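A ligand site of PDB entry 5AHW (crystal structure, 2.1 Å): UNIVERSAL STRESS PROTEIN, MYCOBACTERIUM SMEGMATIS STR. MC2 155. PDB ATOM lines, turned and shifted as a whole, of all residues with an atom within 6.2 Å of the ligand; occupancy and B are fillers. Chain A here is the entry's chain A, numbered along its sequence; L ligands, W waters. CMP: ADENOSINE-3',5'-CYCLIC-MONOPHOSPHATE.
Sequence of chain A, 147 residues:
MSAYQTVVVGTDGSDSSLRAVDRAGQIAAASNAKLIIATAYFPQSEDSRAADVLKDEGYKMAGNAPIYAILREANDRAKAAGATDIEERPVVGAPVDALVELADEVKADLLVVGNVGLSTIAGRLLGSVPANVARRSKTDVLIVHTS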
ATOM      1  N   VAL A   9      20.730 -19.099  10.936  1.00  0.00           N
ATOM      2  CA  VAL A   9      20.878 -18.255  12.165  1.00  0.00           C
ATOM      3  C   VAL A   9      20.715 -16.821  11.764  1.00  0.00           C
ATOM      4  O   VAL A   9      21.205 -16.416  10.710  1.00  0.00           O
ATOM      5  CB  VAL A   9      22.235 -18.466  12.907  1.00  0.00           C
ATOM      6  CG1 VAL A   9      23.482 -18.125  12.126  1.00  0.00           C
ATOM      7  CG2 VAL A   9      22.267 -17.618  14.132  1.00  0.00           C
ATOM      8  N   GLY A  10      19.922 -16.080  12.491  1.00  0.00           N
ATOM      9  CA  GLY A  10      19.791 -14.688  12.222  1.00  0.00           C
ATOM     10  C   GLY A  10      20.731 -13.856  13.061  1.00  0.00           C
ATOM     11  O   GLY A  10      20.832 -14.066  14.270  1.00  0.00           O
ATOM     12  N   THR A  11      21.415 -12.904  12.437  1.00  0.00           N
ATOM     13  CA  THR A  11      22.181 -11.898  13.205  1.00  0.00           C
ATOM     14  C   THR A  11      21.922 -10.478  12.687  1.00  0.00           C
ATOM     15  O   THR A  11      21.773 -10.286  11.488  1.00  0.00           O
ATOM     16  CB  THR A  11      23.686 -12.121  13.121  1.00  0.00           C
ATOM     17  OG1 THR A  11      24.350 -11.010  13.749  1.00  0.00           O
ATOM     18  CG2 THR A  11      24.149 -12.158  11.659  1.00  0.00           C
ATOM     19  N   ASP A  12      21.874  -9.496  13.578  1.00  0.00           N
ATOM     20  CA  ASP A  12      21.793  -8.081  13.232  1.00  0.00           C
ATOM     21  C   ASP A  12      23.129  -7.401  13.531  1.00  0.00           C
ATOM     22  O   ASP A  12      23.256  -6.167  13.476  1.00  0.00           O
ATOM     23  CB  ASP A  12      20.672  -7.355  13.960  1.00  0.00           C
ATOM     24  CG  ASP A  12      20.798  -7.441  15.488  1.00  0.00           C
ATOM     25  OD1 ASP A  12      21.658  -8.197  16.027  1.00  0.00           O
ATOM     26  OD2 ASP A  12      20.015  -6.728  16.132  1.00  0.00           O
ATOM     27  N   SER A  14      24.553  -7.490  16.454  1.00  0.00           N
ATOM     28  CA  SER A  14      24.688  -7.232  17.858  1.00  0.00           C
ATOM     29  C   SER A  14      25.522  -8.330  18.445  1.00  0.00           C
ATOM     30  O   SER A  14      25.492  -9.457  17.954  1.00  0.00           O
ATOM     31  CB  SER A  14      23.311  -7.160  18.550  1.00  0.00           C
ATOM     32  OG  SER A  14      22.624  -8.385  18.393  1.00  0.00           O
ATOM     33  N   ASP A  15      26.212  -7.998  19.532  1.00  0.00           N
ATOM     34  CA  ASP A  15      26.981  -8.933  20.298  1.00  0.00           C
ATOM     35  C   ASP A  15      26.128 -10.027  20.857  1.00  0.00           C
ATOM     36  O   ASP A  15      26.572 -11.131  21.040  1.00  0.00           O
ATOM     37  CB  ASP A  15      27.662  -8.185  21.472  1.00  0.00           C
ATOM     38  CG  ASP A  15      28.832  -7.333  21.028  1.00  0.00           C
ATOM     39  OD1 ASP A  15      29.527  -7.643  20.013  1.00  0.00           O
ATOM     40  OD2 ASP A  15      29.077  -6.332  21.742  1.00  0.00           O
ATOM     41  N   SER A  16      24.867  -9.730  21.175  1.00  0.00           N
ATOM     42  CA  SER A  16      23.980 -10.767  21.678  1.00  0.00           C
ATOM     43  C   SER A  16      23.660 -11.711  20.526  1.00  0.00           C
ATOM     44  O   SER A  16      23.704 -12.903  20.711  1.00  0.00           O
ATOM     45  CB  SER A  16      22.720 -10.167  22.276  1.00  0.00           C
ATOM     46  OG  SER A  16      22.058  -9.365  21.316  1.00  0.00           O
ATOM     47  N   SER A  17      23.290 -11.203  19.368  1.00  0.00           N
ATOM     48  CA  SER A  17      22.985 -12.081  18.253  1.00  0.00           C
ATOM     49  C   SER A  17      24.277 -12.860  17.810  1.00  0.00           C
ATOM     50  O   SER A  17      24.188 -13.968  17.310  1.00  0.00           O
ATOM     51  CB  SER A  17      22.441 -11.255  17.070  1.00  0.00           C
ATOM     52  OG  SER A  17      23.525 -10.716  16.279  1.00  0.00           O
ATOM     53  N   LEU A  18      25.482 -12.367  18.056  1.00  0.00           N
ATOM     54  CA  LEU A  18      26.704 -13.174  17.703  1.00  0.00           C
ATOM     55  C   LEU A  18      26.875 -14.389  18.622  1.00  0.00           C
ATOM     56  O   LEU A  18      27.571 -15.371  18.270  1.00  0.00           O
ATOM     57  CB  LEU A  18      27.962 -12.316  17.778  1.00  0.00           C
ATOM     58  CG  LEU A  18      28.042 -11.237  16.684  1.00  0.00           C
ATOM     59  CD1 LEU A  18      29.158 -10.211  16.910  1.00  0.00           C
ATOM     60  CD2 LEU A  18      28.244 -11.861  15.303  1.00  0.00           C
ATOM     61  N   ARG A  19      26.259 -14.316  19.821  1.00  0.00           N
ATOM     62  CA  ARG A  19      26.312 -15.492  20.698  1.00  0.00           C
ATOM     63  C   ARG A  19      25.351 -16.516  20.123  1.00  0.00           C
ATOM     64  O   ARG A  19      25.598 -17.689  20.209  1.00  0.00           O
ATOM     65  CB  ARG A  19      25.964 -15.198  22.177  1.00  0.00           C
ATOM     66  CG  ARG A  19      27.004 -14.457  22.972  1.00  0.00           C
ATOM     67  CD  ARG A  19      26.477 -13.931  24.340  1.00  0.00           C
ATOM     68  NE  ARG A  19      27.043 -12.597  24.504  1.00  0.00           N
ATOM     69  CZ  ARG A  19      26.414 -11.462  24.788  1.00  0.00           C
ATOM     70  NH1 ARG A  19      25.122 -11.418  25.110  1.00  0.00           N
ATOM     71  NH2 ARG A  19      27.127 -10.340  24.809  1.00  0.00           N
ATOM     72  N   ALA A  20      24.238 -16.068  19.545  1.00  0.00           N
ATOM     73  CA  ALA A  20      23.375 -17.007  18.846  1.00  0.00           C
ATOM     74  C   ALA A  20      24.111 -17.682  17.632  1.00  0.00           C
ATOM     75  O   ALA A  20      23.974 -18.902  17.410  1.00  0.00           O
ATOM     76  CB  ALA A  20      22.146 -16.322  18.369  1.00  0.00           C
ATOM     77  N   ALA A  38      22.026 -15.321   8.135  1.00  0.00           N
ATOM     78  CA  ALA A  38      21.097 -14.411   7.515  1.00  0.00           C
ATOM     79  C   ALA A  38      20.989 -13.129   8.293  1.00  0.00           C
ATOM     80  O   ALA A  38      20.907 -13.138   9.528  1.00  0.00           O
ATOM     81  CB  ALA A  38      19.716 -15.061   7.404  1.00  0.00           C
ATOM     82  N   THR A  39      20.971 -12.028   7.565  1.00  0.00           N
ATOM     83  CA  THR A  39      20.812 -10.705   8.156  1.00  0.00           C
ATOM     84  C   THR A  39      19.759  -9.981   7.317  1.00  0.00           C
ATOM     85  O   THR A  39      19.988  -9.703   6.092  1.00  0.00           O
ATOM     86  CB  THR A  39      22.114  -9.881   8.088  1.00  0.00           C
ATOM     87  OG1 THR A  39      23.161 -10.598   8.744  1.00  0.00           O
ATOM     88  CG2 THR A  39      21.946  -8.551   8.765  1.00  0.00           C
ATOM     89  N   ALA A  40      18.632  -9.646   7.960  1.00  0.00           N
ATOM     90  CA  ALA A  40      17.549  -8.919   7.330  1.00  0.00           C
ATOM     91  C   ALA A  40      17.853  -7.436   7.415  1.00  0.00           C
ATOM     92  O   ALA A  40      18.420  -6.975   8.417  1.00  0.00           O
ATOM     93  CB  ALA A  40      16.258  -9.252   8.043  1.00  0.00           C
ATOM     94  N   TYR A  41      17.515  -6.664   6.388  1.00  0.00           N
ATOM     95  CA  TYR A  41      17.755  -5.222   6.454  1.00  0.00           C
ATOM     96  C   TYR A  41      16.793  -4.493   5.582  1.00  0.00           C
ATOM     97  O   TYR A  41      16.067  -5.112   4.815  1.00  0.00           O
ATOM     98  CB  TYR A  41      19.200  -4.907   6.037  1.00  0.00           C
ATOM     99  CG  TYR A  41      19.462  -5.218   4.572  1.00  0.00           C
ATOM    100  CD1 TYR A  41      19.652  -6.540   4.121  1.00  0.00           C
ATOM    101  CD2 TYR A  41      19.473  -4.203   3.628  1.00  0.00           C
ATOM    102  CE1 TYR A  41      19.850  -6.810   2.777  1.00  0.00           C
ATOM    103  CE2 TYR A  41      19.647  -4.475   2.284  1.00  0.00           C
ATOM    104  CZ  TYR A  41      19.840  -5.770   1.866  1.00  0.00           C
ATOM    105  OH  TYR A  41      20.042  -5.967   0.518  1.00  0.00           O
ATOM    106  N   GLY A  93      13.851  -6.911   4.036  1.00  0.00           N
ATOM    107  CA  GLY A  93      12.597  -6.911   4.764  1.00  0.00           C
ATOM    108  C   GLY A  93      12.755  -6.921   6.280  1.00  0.00           C
ATOM    109  O   GLY A  93      13.857  -6.778   6.840  1.00  0.00           O
ATOM    110  N   PRO A  95      12.872  -8.444   9.984  1.00  0.00           N
ATOM    111  CA  PRO A  95      13.550  -9.612  10.462  1.00  0.00           C
ATOM    112  C   PRO A  95      12.733 -10.905  10.480  1.00  0.00           C
ATOM    113  O   PRO A  95      13.205 -11.921   9.970  1.00  0.00           O
ATOM    114  CB  PRO A  95      13.954  -9.176  11.878  1.00  0.00           C
ATOM    115  CG  PRO A  95      14.319  -7.738  11.648  1.00  0.00           C
ATOM    116  CD  PRO A  95      13.264  -7.239  10.735  1.00  0.00           C
ATOM    117  N   LEU A  99      13.484 -13.986   7.941  1.00  0.00           N
ATOM    118  CA  LEU A  99      13.979 -15.279   8.458  1.00  0.00           C
ATOM    119  C   LEU A  99      13.040 -16.434   8.131  1.00  0.00           C
ATOM    120  O   LEU A  99      13.466 -17.533   7.784  1.00  0.00           O
ATOM    121  CB  LEU A  99      14.190 -15.222   9.985  1.00  0.00           C
ATOM    122  CG  LEU A  99      15.347 -14.356  10.471  1.00  0.00           C
ATOM    123  CD1 LEU A  99      15.413 -14.241  11.952  1.00  0.00           C
ATOM    124  CD2 LEU A  99      16.659 -14.980   9.980  1.00  0.00           C
ATOM    125  N   VAL A 112      17.723 -20.520  14.143  1.00  0.00           N
ATOM    126  CA  VAL A 112      18.347 -20.137  15.384  1.00  0.00           C
ATOM    127  C   VAL A 112      18.305 -18.618  15.558  1.00  0.00           C
ATOM    128  O   VAL A 112      18.737 -17.861  14.660  1.00  0.00           O
ATOM    129  CB  VAL A 112      19.808 -20.632  15.469  1.00  0.00           C
ATOM    130  CG1 VAL A 112      20.327 -20.293  16.873  1.00  0.00           C
ATOM    131  CG2 VAL A 112      19.893 -22.138  15.225  1.00  0.00           C
ATOM    132  N   VAL A 113      17.779 -18.148  16.693  1.00  0.00           N
ATOM    133  CA  VAL A 113      17.773 -16.733  16.995  1.00  0.00           C
ATOM    134  C   VAL A 113      18.183 -16.534  18.468  1.00  0.00           C
ATOM    135  O   VAL A 113      18.053 -17.471  19.287  1.00  0.00           O
ATOM    136  CB  VAL A 113      16.360 -16.244  16.665  1.00  0.00           C
ATOM    137  CG1 VAL A 113      16.136 -14.850  17.138  1.00  0.00           C
ATOM    138  CG2 VAL A 113      16.126 -16.315  15.150  1.00  0.00           C
ATOM    139  N   GLY A 114      18.675 -15.358  18.798  1.00  0.00           N
ATOM    140  CA  GLY A 114      18.854 -14.968  20.204  1.00  0.00           C
ATOM    141  C   GLY A 114      17.546 -14.535  20.847  1.00  0.00           C
ATOM    142  O   GLY A 114      16.446 -14.537  20.221  1.00  0.00           O
ATOM    143  N   ASN A 115      17.626 -14.231  22.140  1.00  0.00           N
ATOM    144  CA  ASN A 115      16.414 -13.936  22.956  1.00  0.00           C
ATOM    145  C   ASN A 115      16.096 -12.471  23.296  1.00  0.00           C
ATOM    146  O   ASN A 115      15.274 -12.244  24.139  1.00  0.00           O
ATOM    147  CB  ASN A 115      16.471 -14.728  24.268  1.00  0.00           C
ATOM    148  CG  ASN A 115      17.480 -14.169  25.242  1.00  0.00           C
ATOM    149  OD1 ASN A 115      18.274 -13.285  24.918  1.00  0.00           O
ATOM    150  ND2 ASN A 115      17.370 -14.590  26.484  1.00  0.00           N
ATOM    151  N   VAL A 116      16.692 -11.470  22.645  1.00  0.00           N
ATOM    152  CA  VAL A 116      16.432 -10.088  23.022  1.00  0.00           C
ATOM    153  C   VAL A 116      14.952  -9.755  22.804  1.00  0.00           C
ATOM    154  O   VAL A 116      14.308 -10.129  21.801  1.00  0.00           O
ATOM    155  CB  VAL A 116      17.363  -9.034  22.404  1.00  0.00           C
ATOM    156  CG1 VAL A 116      16.946  -7.615  22.787  1.00  0.00           C
ATOM    157  CG2 VAL A 116      18.827  -9.230  22.805  1.00  0.00           C
ATOM    158  N   GLY A 117      14.388  -9.151  23.853  1.00  0.00           N
ATOM    159  CA  GLY A 117      12.984  -8.772  23.807  1.00  0.00           C
ATOM    160  C   GLY A 117      11.979  -9.833  24.274  1.00  0.00           C
ATOM    161  O   GLY A 117      10.851  -9.509  24.669  1.00  0.00           O
ATOM    162  N   VAL A 129      11.499 -10.559  17.919  1.00  0.00           N
ATOM    163  CA  VAL A 129      11.914 -11.541  16.925  1.00  0.00           C
ATOM    164  C   VAL A 129      11.758 -12.975  17.364  1.00  0.00           C
ATOM    165  O   VAL A 129      11.127 -13.768  16.705  1.00  0.00           O
ATOM    166  CB  VAL A 129      13.301 -11.177  16.384  1.00  0.00           C
ATOM    167  CG1 VAL A 129      13.691 -12.095  15.213  1.00  0.00           C
ATOM    168  CG2 VAL A 129      13.239  -9.753  15.855  1.00  0.00           C
ATOM    169  N   PRO A 130      12.284 -13.342  18.524  1.00  0.00           N
ATOM    170  CA  PRO A 130      12.200 -14.747  18.851  1.00  0.00           C
ATOM    171  C   PRO A 130      10.834 -15.269  19.055  1.00  0.00           C
ATOM    172  O   PRO A 130      10.565 -16.349  18.640  1.00  0.00           O
ATOM    173  CB  PRO A 130      13.027 -14.872  20.159  1.00  0.00           C
ATOM    174  CG  PRO A 130      13.255 -13.467  20.595  1.00  0.00           C
ATOM    175  CD  PRO A 130      13.301 -12.658  19.346  1.00  0.00           C
ATOM    176  N   VAL A 144      18.303 -18.990  21.615  1.00  0.00           N
ATOM    177  CA  VAL A 144      19.531 -19.021  22.445  1.00  0.00           C
ATOM    178  C   VAL A 144      19.410 -17.946  23.505  1.00  0.00           C
ATOM    179  O   VAL A 144      19.038 -16.823  23.201  1.00  0.00           O
ATOM    180  CB  VAL A 144      20.780 -18.739  21.602  1.00  0.00           C
ATOM    181  CG1 VAL A 144      22.072 -18.851  22.415  1.00  0.00           C
ATOM    182  CG2 VAL A 144      20.847 -19.761  20.476  1.00  0.00           C
ATOM    183  N   THR A 146      20.868 -15.413  24.962  1.00  0.00           N
ATOM    184  CA  THR A 146      22.004 -14.636  24.665  1.00  0.00           C
ATOM    185  C   THR A 146      22.116 -13.438  25.531  1.00  0.00           C
ATOM    186  O   THR A 146      23.163 -12.828  25.573  1.00  0.00           O
ATOM    187  CB  THR A 146      21.917 -14.069  23.265  1.00  0.00           C
ATOM    188  OG1 THR A 146      20.666 -13.443  23.098  1.00  0.00           O
ATOM    189  CG2 THR A 146      22.044 -15.181  22.256  1.00  0.00           C
ATOM    190  N   SER A 147      21.066 -13.077  26.223  1.00  0.00           N
ATOM    191  CA  SER A 147      21.095 -11.932  27.141  1.00  0.00           C
ATOM    192  C   SER A 147      20.175 -12.209  28.368  1.00  0.00           C
ATOM    193  O   SER A 147      19.382 -13.161  28.360  1.00  0.00           O
ATOM    194  CB  SER A 147      20.595 -10.696  26.445  1.00  0.00           C
ATOM    195  OG  SER A 147      19.225 -10.910  26.091  1.00  0.00           O
ATOM    196  OXT SER A 147      20.248 -11.557  29.393  1.00  0.00           O
HETATM  197  P   CMP L   1      19.842 -11.385  19.742  1.00  0.00           P
HETATM  198  O1P CMP L   1      20.517 -12.279  20.750  1.00  0.00           O
HETATM  199  O2P CMP L   1      20.119  -9.952  19.648  1.00  0.00           O
HETATM  200  O5' CMP L   1      18.282 -11.358  20.129  1.00  0.00           O
HETATM  201  C5' CMP L   1      17.269 -11.090  19.188  1.00  0.00           C
HETATM  202  C4' CMP L   1      17.546 -11.981  17.980  1.00  0.00           C
HETATM  203  O4' CMP L   1      16.693 -11.762  16.911  1.00  0.00           O
HETATM  204  C3' CMP L   1      18.928 -11.697  17.397  1.00  0.00           C
HETATM  205  O3' CMP L   1      19.826 -12.204  18.354  1.00  0.00           O
HETATM  206  C2' CMP L   1      18.802 -12.338  16.039  1.00  0.00           C
HETATM  207  O2' CMP L   1      18.969 -13.731  16.044  1.00  0.00           O
HETATM  208  C1' CMP L   1      17.370 -11.944  15.662  1.00  0.00           C
HETATM  209  N9  CMP L   1      17.382 -10.690  14.869  1.00  0.00           N
HETATM  210  C8  CMP L   1      17.123  -9.456  15.258  1.00  0.00           C
HETATM  211  N7  CMP L   1      17.263  -8.589  14.223  1.00  0.00           N
HETATM  212  C5  CMP L   1      17.633  -9.278  13.148  1.00  0.00           C
HETATM  213  C6  CMP L   1      18.032  -9.036  11.721  1.00  0.00           C
HETATM  214  N6  CMP L   1      18.012  -7.843  11.165  1.00  0.00           N
HETATM  215  N1  CMP L   1      18.409 -10.054  10.947  1.00  0.00           N
HETATM  216  C2  CMP L   1      18.403 -11.305  11.404  1.00  0.00           C
HETATM  217  N3  CMP L   1      18.127 -11.594  12.685  1.00  0.00           N
HETATM  218  C4  CMP L   1      17.737 -10.645  13.592  1.00  0.00           C
HETATM  219  O   HOH W   1      16.309  -7.804  18.069  1.00  0.00           O
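An oxygen (O2') of the ligand sits at hydrogen-bond distance from the backbone carbonyl oxygen (O) of Gly 10 (2.6 Å). O2P of the ligand lies within hydrogen-bond range of OG of Ser 16 (2.6 Å). The side-chain hydroxyl (OG1) of Thr 146 sits at hydrogen-bond distance from an oxygen (O1P) of the ligand. N1 of the ligand lies within hydrogen-bond range of N of Ala 40. O of Ala 40 sits at hydrogen-bond distance from N6 of the ligand, at 2.9 Å. An oxygen (O5') of the ligand lies within hydrogen-bond range of the backbone NH (N) of Val 116 (3.0 Å). N of Ser 17 sits at hydrogen-bond distance from O1P of the ligand. O2' of the ligand is in hydrogen-bond range of N of Gly 114 (3.2 Å). OG of Ser 14 is in hydrogen-bond range of O2P of the ligand (3.2 Å).
O of Thr 11 lies close to N1 of the ligand. Residues that only touch the ligand: Val 113, Val 129, Asn 115, Ala 38, Asp 12, Pro 95, Thr 39 and Leu 99. Of the 29 residues printed, 17 come within 4 Å of the ligand.
OG of Ser 16 is in hydrogen-bond range of OG of Ser 14 (3.1 Å). OG1 of Thr 146 sits at hydrogen-bond distance from OD1 of Asn 115, 3.0 Å away. The backbone carbonyl oxygen (O) of Ser 14 lies within hydrogen-bond range of the side-chain hydroxyl (OG) of Ser 17 (2.9 Å). The side-chain hydroxyl (OG) of Ser 17 sits at hydrogen-bond distance from the side-chain hydroxyl (OG1) of Thr 11 (2.7 Å). The side-chain hydroxyl of Ser 17 sits at hydrogen-bond distance from the side-chain carboxylate of Asp 12, at 3.1 Å. The backbone carbonyl oxygen (O) of Val 113 lies within hydrogen-bond range of the backbone NH (N) of Val 144. O of Ala 38 sits at hydrogen-bond distance from N of Thr 11. N of Ala 38 lies within hydrogen-bond range of O of Val 9 (2.9 Å).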
